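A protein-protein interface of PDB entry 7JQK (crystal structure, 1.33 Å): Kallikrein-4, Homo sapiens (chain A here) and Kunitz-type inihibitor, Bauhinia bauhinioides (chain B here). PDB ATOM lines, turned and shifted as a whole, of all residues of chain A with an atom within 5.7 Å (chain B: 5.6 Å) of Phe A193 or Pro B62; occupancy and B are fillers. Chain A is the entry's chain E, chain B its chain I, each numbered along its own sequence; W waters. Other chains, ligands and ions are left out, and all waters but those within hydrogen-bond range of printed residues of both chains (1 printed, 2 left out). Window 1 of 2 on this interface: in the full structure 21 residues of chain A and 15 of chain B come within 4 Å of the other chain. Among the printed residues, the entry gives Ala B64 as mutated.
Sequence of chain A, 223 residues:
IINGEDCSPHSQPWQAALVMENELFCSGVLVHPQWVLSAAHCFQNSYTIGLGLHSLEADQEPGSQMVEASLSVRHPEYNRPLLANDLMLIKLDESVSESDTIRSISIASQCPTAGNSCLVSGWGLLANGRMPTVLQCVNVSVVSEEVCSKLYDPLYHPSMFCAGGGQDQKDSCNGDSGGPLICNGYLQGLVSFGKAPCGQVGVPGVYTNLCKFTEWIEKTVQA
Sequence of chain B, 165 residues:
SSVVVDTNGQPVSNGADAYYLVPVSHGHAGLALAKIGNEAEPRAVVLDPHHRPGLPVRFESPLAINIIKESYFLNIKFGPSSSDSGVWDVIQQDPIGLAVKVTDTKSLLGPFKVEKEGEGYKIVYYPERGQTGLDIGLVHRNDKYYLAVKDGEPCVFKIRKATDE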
ATOM      1  N   HIS A  41      -7.932  26.463  16.975  1.00  0.00           N
ATOM      2  CA  HIS A  41      -7.361  26.156  18.284  1.00  0.00           C
ATOM      3  C   HIS A  41      -6.485  27.304  18.822  1.00  0.00           C
ATOM      4  O   HIS A  41      -6.091  27.256  19.992  1.00  0.00           O
ATOM      5  CB  HIS A  41      -6.620  24.803  18.263  1.00  0.00           C
ATOM      6  CG  HIS A  41      -5.317  24.841  17.544  1.00  0.00           C
ATOM      7  ND1 HIS A  41      -5.159  24.390  16.223  1.00  0.00           N
ATOM      8  CD2 HIS A  41      -4.049  25.187  17.960  1.00  0.00           C
ATOM      9  CE1 HIS A  41      -3.857  24.441  15.897  1.00  0.00           C
ATOM     10  NE2 HIS A  41      -3.132  24.951  16.917  1.00  0.00           N
ATOM     11  N   LEU A  83     -10.583  17.667  16.536  1.00  0.00           N
ATOM     12  CA  LEU A  83      -9.498  18.242  15.744  1.00  0.00           C
ATOM     13  C   LEU A  83      -9.949  18.768  14.388  1.00  0.00           C
ATOM     14  O   LEU A  83      -9.146  19.463  13.728  1.00  0.00           O
ATOM     15  CB  LEU A  83      -8.278  17.303  15.546  1.00  0.00           C
ATOM     16  CG  LEU A  83      -7.705  16.734  16.852  1.00  0.00           C
ATOM     17  CD1 LEU A  83      -6.573  15.792  16.524  1.00  0.00           C
ATOM     18  CD2 LEU A  83      -7.235  17.843  17.772  1.00  0.00           C
ATOM     19  N   ASP A  86     -10.645  23.065  11.601  1.00  0.00           N
ATOM     20  CA  ASP A  86      -9.762  23.868  12.463  1.00  0.00           C
ATOM     21  C   ASP A  86      -9.409  25.192  11.782  1.00  0.00           C
ATOM     22  O   ASP A  86      -8.289  25.369  11.263  1.00  0.00           O
ATOM     23  CB  ASP A  86      -8.518  23.036  12.808  1.00  0.00           C
ATOM     24  CG  ASP A  86      -7.661  23.697  13.905  1.00  0.00           C
ATOM     25  OD1 ASP A  86      -8.083  24.729  14.500  1.00  0.00           O
ATOM     26  OD2 ASP A  86      -6.553  23.173  14.177  1.00  0.00           O
ATOM     27  N   TYR A 152      -4.034   8.382  10.180  1.00  0.00           N
ATOM     28  CA  TYR A 152      -4.662   9.230  11.210  1.00  0.00           C
ATOM     29  C   TYR A 152      -6.071   8.779  11.572  1.00  0.00           C
ATOM     30  O   TYR A 152      -6.548   9.253  12.608  1.00  0.00           O
ATOM     31  CB  TYR A 152      -4.679  10.705  10.766  1.00  0.00           C
ATOM     32  CG  TYR A 152      -3.331  11.346  10.999  1.00  0.00           C
ATOM     33  CD1 TYR A 152      -2.957  11.764  12.265  1.00  0.00           C
ATOM     34  CD2 TYR A 152      -2.448  11.577   9.932  1.00  0.00           C
ATOM     35  CE1 TYR A 152      -1.718  12.355  12.492  1.00  0.00           C
ATOM     36  CE2 TYR A 152      -1.218  12.167  10.127  1.00  0.00           C
ATOM     37  CZ  TYR A 152      -0.848  12.557  11.423  1.00  0.00           C
ATOM     38  OH  TYR A 152       0.342  13.216  11.669  1.00  0.00           O
ATOM     39  N   LEU A 155      -9.178   9.858  13.462  1.00  0.00           N
ATOM     40  CA  LEU A 155      -9.260  11.314  13.581  1.00  0.00           C
ATOM     41  C   LEU A 155      -9.103  11.988  12.207  1.00  0.00           C
ATOM     42  O   LEU A 155      -9.164  13.225  12.152  1.00  0.00           O
ATOM     43  CB  LEU A 155      -8.220  11.806  14.587  1.00  0.00           C
ATOM     44  CG  LEU A 155      -8.516  11.410  16.019  1.00  0.00           C
ATOM     45  CD1 LEU A 155      -7.370  11.823  16.960  1.00  0.00           C
ATOM     46  CD2 LEU A 155      -9.883  11.988  16.446  1.00  0.00           C
ATOM     47  N   MET A 160      -9.285  18.116   6.669  1.00  0.00           N
ATOM     48  CA  MET A 160      -7.838  18.011   6.893  1.00  0.00           C
ATOM     49  C   MET A 160      -7.202  17.486   5.599  1.00  0.00           C
ATOM     50  O   MET A 160      -7.853  16.756   4.822  1.00  0.00           O
ATOM     51  CB  MET A 160      -7.547  16.947   7.968  1.00  0.00           C
ATOM     52  CG  MET A 160      -8.248  17.273   9.304  1.00  0.00           C
ATOM     53  SD  MET A 160      -8.112  15.763  10.332  1.00  0.00           S
ATOM     54  CE  MET A 160      -9.062  16.317  11.778  1.00  0.00           C
ATOM     55  N   ASN A 174       5.890  22.789  16.679  1.00  0.00           N
ATOM     56  CA  ASN A 174       5.138  23.584  17.635  1.00  0.00           C
ATOM     57  C   ASN A 174       5.476  25.075  17.518  1.00  0.00           C
ATOM     58  O   ASN A 174       6.655  25.443  17.500  1.00  0.00           O
ATOM     59  CB  ASN A 174       5.376  23.069  19.057  1.00  0.00           C
ATOM     60  CG  ASN A 174       4.901  21.632  19.170  1.00  0.00           C
ATOM     61  OD1 ASN A 174       3.767  21.338  19.554  1.00  0.00           O
ATOM     62  ND2 ASN A 174       5.713  20.728  18.707  1.00  0.00           N
ATOM     63  N   VAL A 191      -1.400  25.261   9.123  1.00  0.00           N
ATOM     64  CA  VAL A 191      -0.784  24.292  10.025  1.00  0.00           C
ATOM     65  C   VAL A 191      -1.759  23.953  11.160  1.00  0.00           C
ATOM     66  O   VAL A 191      -2.228  24.866  11.846  1.00  0.00           O
ATOM     67  CB  VAL A 191       0.518  24.874  10.604  1.00  0.00           C
ATOM     68  CG1 VAL A 191       1.159  23.876  11.582  1.00  0.00           C
ATOM     69  CG2 VAL A 191       1.537  25.210   9.488  1.00  0.00           C
ATOM     70  N   SER A 192      -2.027  22.648  11.399  1.00  0.00           N
ATOM     71  CA  SER A 192      -3.033  22.294  12.405  1.00  0.00           C
ATOM     72  C   SER A 192      -2.425  21.365  13.470  1.00  0.00           C
ATOM     73  O   SER A 192      -2.318  21.789  14.644  1.00  0.00           O
ATOM     74  CB  SER A 192      -4.265  21.677  11.687  1.00  0.00           C
ATOM     75  OG  SER A 192      -5.254  21.314  12.685  1.00  0.00           O
ATOM     76  N   PHE A 193      -2.050  20.112  13.140  1.00  0.00           N
ATOM     77  CA  PHE A 193      -1.614  19.189  14.194  1.00  0.00           C
ATOM     78  C   PHE A 193      -0.730  18.104  13.607  1.00  0.00           C
ATOM     79  O   PHE A 193      -0.628  17.995  12.362  1.00  0.00           O
ATOM     80  CB  PHE A 193      -2.804  18.594  15.014  1.00  0.00           C
ATOM     81  CG  PHE A 193      -3.653  17.594  14.250  1.00  0.00           C
ATOM     82  CD1 PHE A 193      -4.734  18.027  13.473  1.00  0.00           C
ATOM     83  CD2 PHE A 193      -3.355  16.230  14.296  1.00  0.00           C
ATOM     84  CE1 PHE A 193      -5.567  17.124  12.801  1.00  0.00           C
ATOM     85  CE2 PHE A 193      -4.155  15.302  13.615  1.00  0.00           C
ATOM     86  CZ  PHE A 193      -5.257  15.761  12.882  1.00  0.00           C
ATOM     87  N   GLY A 194      -0.152  17.254  14.446  1.00  0.00           N
ATOM     88  CA  GLY A 194       0.607  16.124  13.927  1.00  0.00           C
ATOM     89  C   GLY A 194       1.072  15.228  15.059  1.00  0.00           C
ATOM     90  O   GLY A 194       0.827  15.499  16.207  1.00  0.00           O
ATOM     91  N   LYS A 195       1.749  14.153  14.707  1.00  0.00           N
ATOM     92  CA  LYS A 195       2.336  13.272  15.696  1.00  0.00           C
ATOM     93  C   LYS A 195       3.685  13.829  16.140  1.00  0.00           C
ATOM     94  O   LYS A 195       4.431  14.385  15.373  1.00  0.00           O
ATOM     95  CB  LYS A 195       2.524  11.875  15.108  1.00  0.00           C
ATOM     96  CG  LYS A 195       2.944  10.845  16.149  1.00  0.00           C
ATOM     97  CD  LYS A 195       3.041   9.397  15.709  1.00  0.00           C
ATOM     98  CE  LYS A 195       3.808   8.628  16.765  1.00  0.00           C
ATOM     99  NZ  LYS A 195       3.331   7.236  16.890  1.00  0.00           N
ATOM    100  N   PRO A 204       3.554  12.381   8.021  1.00  0.00           N
ATOM    101  CA  PRO A 204       3.237  13.741   7.570  1.00  0.00           C
ATOM    102  C   PRO A 204       2.514  14.497   8.691  1.00  0.00           C
ATOM    103  O   PRO A 204       1.930  13.887   9.606  1.00  0.00           O
ATOM    104  CB  PRO A 204       2.315  13.509   6.371  1.00  0.00           C
ATOM    105  CG  PRO A 204       1.679  12.160   6.626  1.00  0.00           C
ATOM    106  CD  PRO A 204       2.623  11.371   7.505  1.00  0.00           C
ATOM    107  N   GLY A 205       2.549  15.816   8.600  1.00  0.00           N
ATOM    108  CA  GLY A 205       1.738  16.697   9.438  1.00  0.00           C
ATOM    109  C   GLY A 205       0.352  16.882   8.821  1.00  0.00           C
ATOM    110  O   GLY A 205       0.127  16.607   7.621  1.00  0.00           O
ATOM    111  N   VAL A 206      -0.563  17.420   9.623  1.00  0.00           N
ATOM    112  CA  VAL A 206      -1.952  17.617   9.206  1.00  0.00           C
ATOM    113  C   VAL A 206      -2.266  19.112   9.143  1.00  0.00           C
ATOM    114  O   VAL A 206      -1.899  19.908  10.033  1.00  0.00           O
ATOM    115  CB  VAL A 206      -2.955  16.869  10.127  1.00  0.00           C
ATOM    116  CG1 VAL A 206      -4.363  16.961   9.548  1.00  0.00           C
ATOM    117  CG2 VAL A 206      -2.486  15.408  10.258  1.00  0.00           C
ATOM    118  N   TYR A 207      -2.961  19.499   8.043  1.00  0.00           N
ATOM    119  CA  TYR A 207      -3.252  20.886   7.708  1.00  0.00           C
ATOM    120  C   TYR A 207      -4.739  21.074   7.500  1.00  0.00           C
ATOM    121  O   TYR A 207      -5.412  20.164   7.011  1.00  0.00           O
ATOM    122  CB  TYR A 207      -2.496  21.268   6.413  1.00  0.00           C
ATOM    123  CG  TYR A 207      -0.998  21.232   6.592  1.00  0.00           C
ATOM    124  CD1 TYR A 207      -0.307  20.022   6.570  1.00  0.00           C
ATOM    125  CD2 TYR A 207      -0.299  22.407   6.877  1.00  0.00           C
ATOM    126  CE1 TYR A 207       1.072  19.933   6.816  1.00  0.00           C
ATOM    127  CE2 TYR A 207       1.092  22.372   7.094  1.00  0.00           C
ATOM    128  CZ  TYR A 207       1.752  21.137   7.091  1.00  0.00           C
ATOM    129  OH  TYR A 207       3.094  21.128   7.366  1.00  0.00           O
ATOM    130  N   ASN B  14       3.681  23.000  25.598  1.00  0.00           N
ATOM    131  CA  ASN B  14       3.152  21.767  25.009  1.00  0.00           C
ATOM    132  C   ASN B  14       4.317  20.781  24.884  1.00  0.00           C
ATOM    133  O   ASN B  14       5.048  20.778  23.870  1.00  0.00           O
ATOM    134  CB  ASN B  14       2.446  22.115  23.689  1.00  0.00           C
ATOM    135  CG  ASN B  14       1.897  20.874  23.019  1.00  0.00           C
ATOM    136  OD1 ASN B  14       1.936  19.784  23.606  1.00  0.00           O
ATOM    137  ND2 ASN B  14       1.312  21.073  21.820  1.00  0.00           N
ATOM    138  N   GLU B  60       0.872  17.105  26.857  1.00  0.00           N
ATOM    139  CA  GLU B  60       1.095  17.072  25.421  1.00  0.00           C
ATOM    140  C   GLU B  60      -0.242  17.108  24.680  1.00  0.00           C
ATOM    141  O   GLU B  60      -1.180  16.357  24.973  1.00  0.00           O
ATOM    142  CB  GLU B  60       1.785  15.734  25.043  1.00  0.00           C
ATOM    143  CG  GLU B  60       3.200  15.582  25.595  1.00  0.00           C
ATOM    144  CD  GLU B  60       3.946  14.299  25.192  1.00  0.00           C
ATOM    145  OE1 GLU B  60       3.292  13.355  24.794  1.00  0.00           O
ATOM    146  OE2 GLU B  60       5.193  14.303  25.164  1.00  0.00           O
ATOM    147  N   SER B  61      -0.285  17.924  23.621  1.00  0.00           N
ATOM    148  CA  SER B  61      -1.397  17.992  22.674  1.00  0.00           C
ATOM    149  C   SER B  61      -0.754  17.842  21.285  1.00  0.00           C
ATOM    150  O   SER B  61       0.344  18.350  21.036  1.00  0.00           O
ATOM    151  CB  SER B  61      -2.004  19.387  22.761  1.00  0.00           C
ATOM    152  OG  SER B  61      -2.829  19.640  21.602  1.00  0.00           O
ATOM    153  N   PRO B  62      -1.438  17.194  20.325  1.00  0.00           N
ATOM    154  CA  PRO B  62      -0.891  17.076  18.957  1.00  0.00           C
ATOM    155  C   PRO B  62      -0.940  18.403  18.215  1.00  0.00           C
ATOM    156  O   PRO B  62      -0.357  18.496  17.133  1.00  0.00           O
ATOM    157  CB  PRO B  62      -1.806  16.034  18.318  1.00  0.00           C
ATOM    158  CG  PRO B  62      -3.140  16.237  19.028  1.00  0.00           C
ATOM    159  CD  PRO B  62      -2.767  16.509  20.485  1.00  0.00           C
ATOM    160  N   LEU B  63      -1.694  19.408  18.720  1.00  0.00           N
ATOM    161  CA  LEU B  63      -1.795  20.677  18.008  1.00  0.00           C
ATOM    162  C   LEU B  63      -0.393  21.307  17.901  1.00  0.00           C
ATOM    163  O   LEU B  63       0.427  21.212  18.817  1.00  0.00           O
ATOM    164  CB  LEU B  63      -2.692  21.613  18.827  1.00  0.00           C
ATOM    165  CG  LEU B  63      -4.133  21.096  18.973  1.00  0.00           C
ATOM    166  CD1 LEU B  63      -4.907  21.965  20.006  1.00  0.00           C
ATOM    167  CD2 LEU B  63      -4.881  21.054  17.618  1.00  0.00           C
ATOM    168  N   ALA B  64      -0.144  22.003  16.767  1.00  0.00           N
ATOM    169  CA  ALA B  64       1.193  22.545  16.485  1.00  0.00           C
ATOM    170  C   ALA B  64       1.462  23.884  17.189  1.00  0.00           C
ATOM    171  O   ALA B  64       2.058  24.813  16.622  1.00  0.00           O
ATOM    172  CB  ALA B  64       1.364  22.665  14.965  1.00  0.00           C
ATOM    173  N   PHE B  73      -7.644  18.520  24.840  1.00  0.00           N
ATOM    174  CA  PHE B  73      -7.368  17.150  25.315  1.00  0.00           C
ATOM    175  C   PHE B  73      -5.857  16.890  25.362  1.00  0.00           C
ATOM    176  O   PHE B  73      -5.140  17.193  24.378  1.00  0.00           O
ATOM    177  CB  PHE B  73      -7.993  16.121  24.383  1.00  0.00           C
ATOM    178  CG  PHE B  73      -9.427  15.849  24.746  1.00  0.00           C
ATOM    179  CD1 PHE B  73      -9.710  15.345  26.025  1.00  0.00           C
ATOM    180  CD2 PHE B  73     -10.462  16.057  23.827  1.00  0.00           C
ATOM    181  CE1 PHE B  73     -11.013  15.076  26.372  1.00  0.00           C
ATOM    182  CE2 PHE B  73     -11.790  15.735  24.161  1.00  0.00           C
ATOM    183  CZ  PHE B  73     -12.032  15.219  25.451  1.00  0.00           C
ATOM    184  N   LEU B 108      -2.716   9.511  20.028  1.00  0.00           N
ATOM    185  CA  LEU B 108      -2.436  10.827  19.492  1.00  0.00           C
ATOM    186  C   LEU B 108      -3.042  11.916  20.364  1.00  0.00           C
ATOM    187  O   LEU B 108      -2.459  12.998  20.549  1.00  0.00           O
ATOM    188  CB  LEU B 108      -2.961  10.929  18.046  1.00  0.00           C
ATOM    189  CG  LEU B 108      -2.652  12.249  17.358  1.00  0.00           C
ATOM    190  CD1 LEU B 108      -1.146  12.466  17.132  1.00  0.00           C
ATOM    191  CD2 LEU B 108      -3.346  12.270  16.003  1.00  0.00           C
ATOM    192  N   LEU B 109      -4.269  11.680  20.814  1.00  0.00           N
ATOM    193  CA  LEU B 109      -5.006  12.652  21.627  1.00  0.00           C
ATOM    194  C   LEU B 109      -5.352  11.973  22.949  1.00  0.00           C
ATOM    195  O   LEU B 109      -6.021  10.920  23.004  1.00  0.00           O
ATOM    196  CB  LEU B 109      -6.208  12.985  20.728  1.00  0.00           C
ATOM    197  CG  LEU B 109      -6.996  14.191  21.145  1.00  0.00           C
ATOM    198  CD1 LEU B 109      -6.166  15.481  21.118  1.00  0.00           C
ATOM    199  CD2 LEU B 109      -8.264  14.295  20.296  1.00  0.00           C
HETATM  200  O   HOH W   1       2.707  18.642  19.526  1.00  0.00           O
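The side-chain amide oxygen (OD1) of Asn A174 lies within hydrogen-bond range of the side-chain amide nitrogen (ND2) of Asn B14 (3.4 Å). O of Leu B63 sits close to OD1 of Asn A174, at 3.4 Å. The backbone carbonyl oxygen (O) of Ser A192 lies within hydrogen-bond range of the backbone NH (N) of Ala B64 (3.0 Å). N of Gly A194 lies within hydrogen-bond range of O of Pro B62 (3.0 Å).
The side-chain hydroxyl of Ser A192 sits at hydrogen-bond distance from the side-chain carboxylate of Asp A86 (2.7 Å). OH of Tyr A152 sits at hydrogen-bond distance from N of Lys A195 (3.5 Å). OH of Tyr A152 lies within hydrogen-bond range of O of Pro A204 (2.7 Å). The backbone carbonyl oxygen of Val A206 lies within hydrogen-bond range of the backbone NH of Ser A192 (3.1 Å). OD1 of Asn B14 sits at hydrogen-bond distance from N of Ser B61 (2.9 Å). The side-chain amide nitrogen of Asn B14 is in hydrogen-bond range of the backbone carbonyl oxygen of Leu B63 (3.1 Å).
Leu A83 touches Leu B63 (CD2 to CD2, 3.98 Å). CD1 of Tyr A152 touches CD2 of Leu B108, at 3.8 Å. Ala B64 touches Asn A174. Val A191 touches Ala B64. CA of Leu B63 touches O of Ser A192, 3.6 Å away. O of Pro B62 touches CB of Phe A193, 3.2 Å away. Phe A193 touches Leu B63. CE2 of Phe A193 touches CD2 of Leu B108, 3.9 Å away. O of Gly A194 touches CD1 of Leu B108, at 3.7 Å. CD1 of Leu B108 touches CA of Lys A195, 3.9 Å away.
Phe A193 touches just these residues of chain B: Pro B62 (3.2 Å), Leu B63 (3.8 Å) and Leu B108 (3.9 Å). Pro B62 touches two residues of chain A. Of the printed residues of chain A, Ala B64 touches Asn A174 (3.5 Å), Val A191 (3.6 Å) and Ser A192 (3.0 Å). Printed residues of chain B within 4 Å of His A41: Leu B63. Glu B60 touches none of the printed residues of chain A. The nearest residue of chain B that does not touch Phe A193 is Ala B64 (4.1 Å). The nearest printed residue of chain B that does not touch Lys A195 is Pro B62 (5.4 Å).
Printed residues of chain B that touch a printed residue of chain A: Asn B14, Pro B62, Leu B63, Ala B64 and Leu B108. Of the 16 printed residues of chain A, 9 touch a printed residue of chain B. Hydrophobic or aromatic side chains of chain A that line the printed part of chain B: His A41, Leu A83, Tyr A152, Val A191 and Phe A193.
Water W1 lies within hydrogen-bond range of the backbone carbonyl oxygen (O) of Ser B61 and the side-chain amide oxygen (OD1) of Asn A174.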
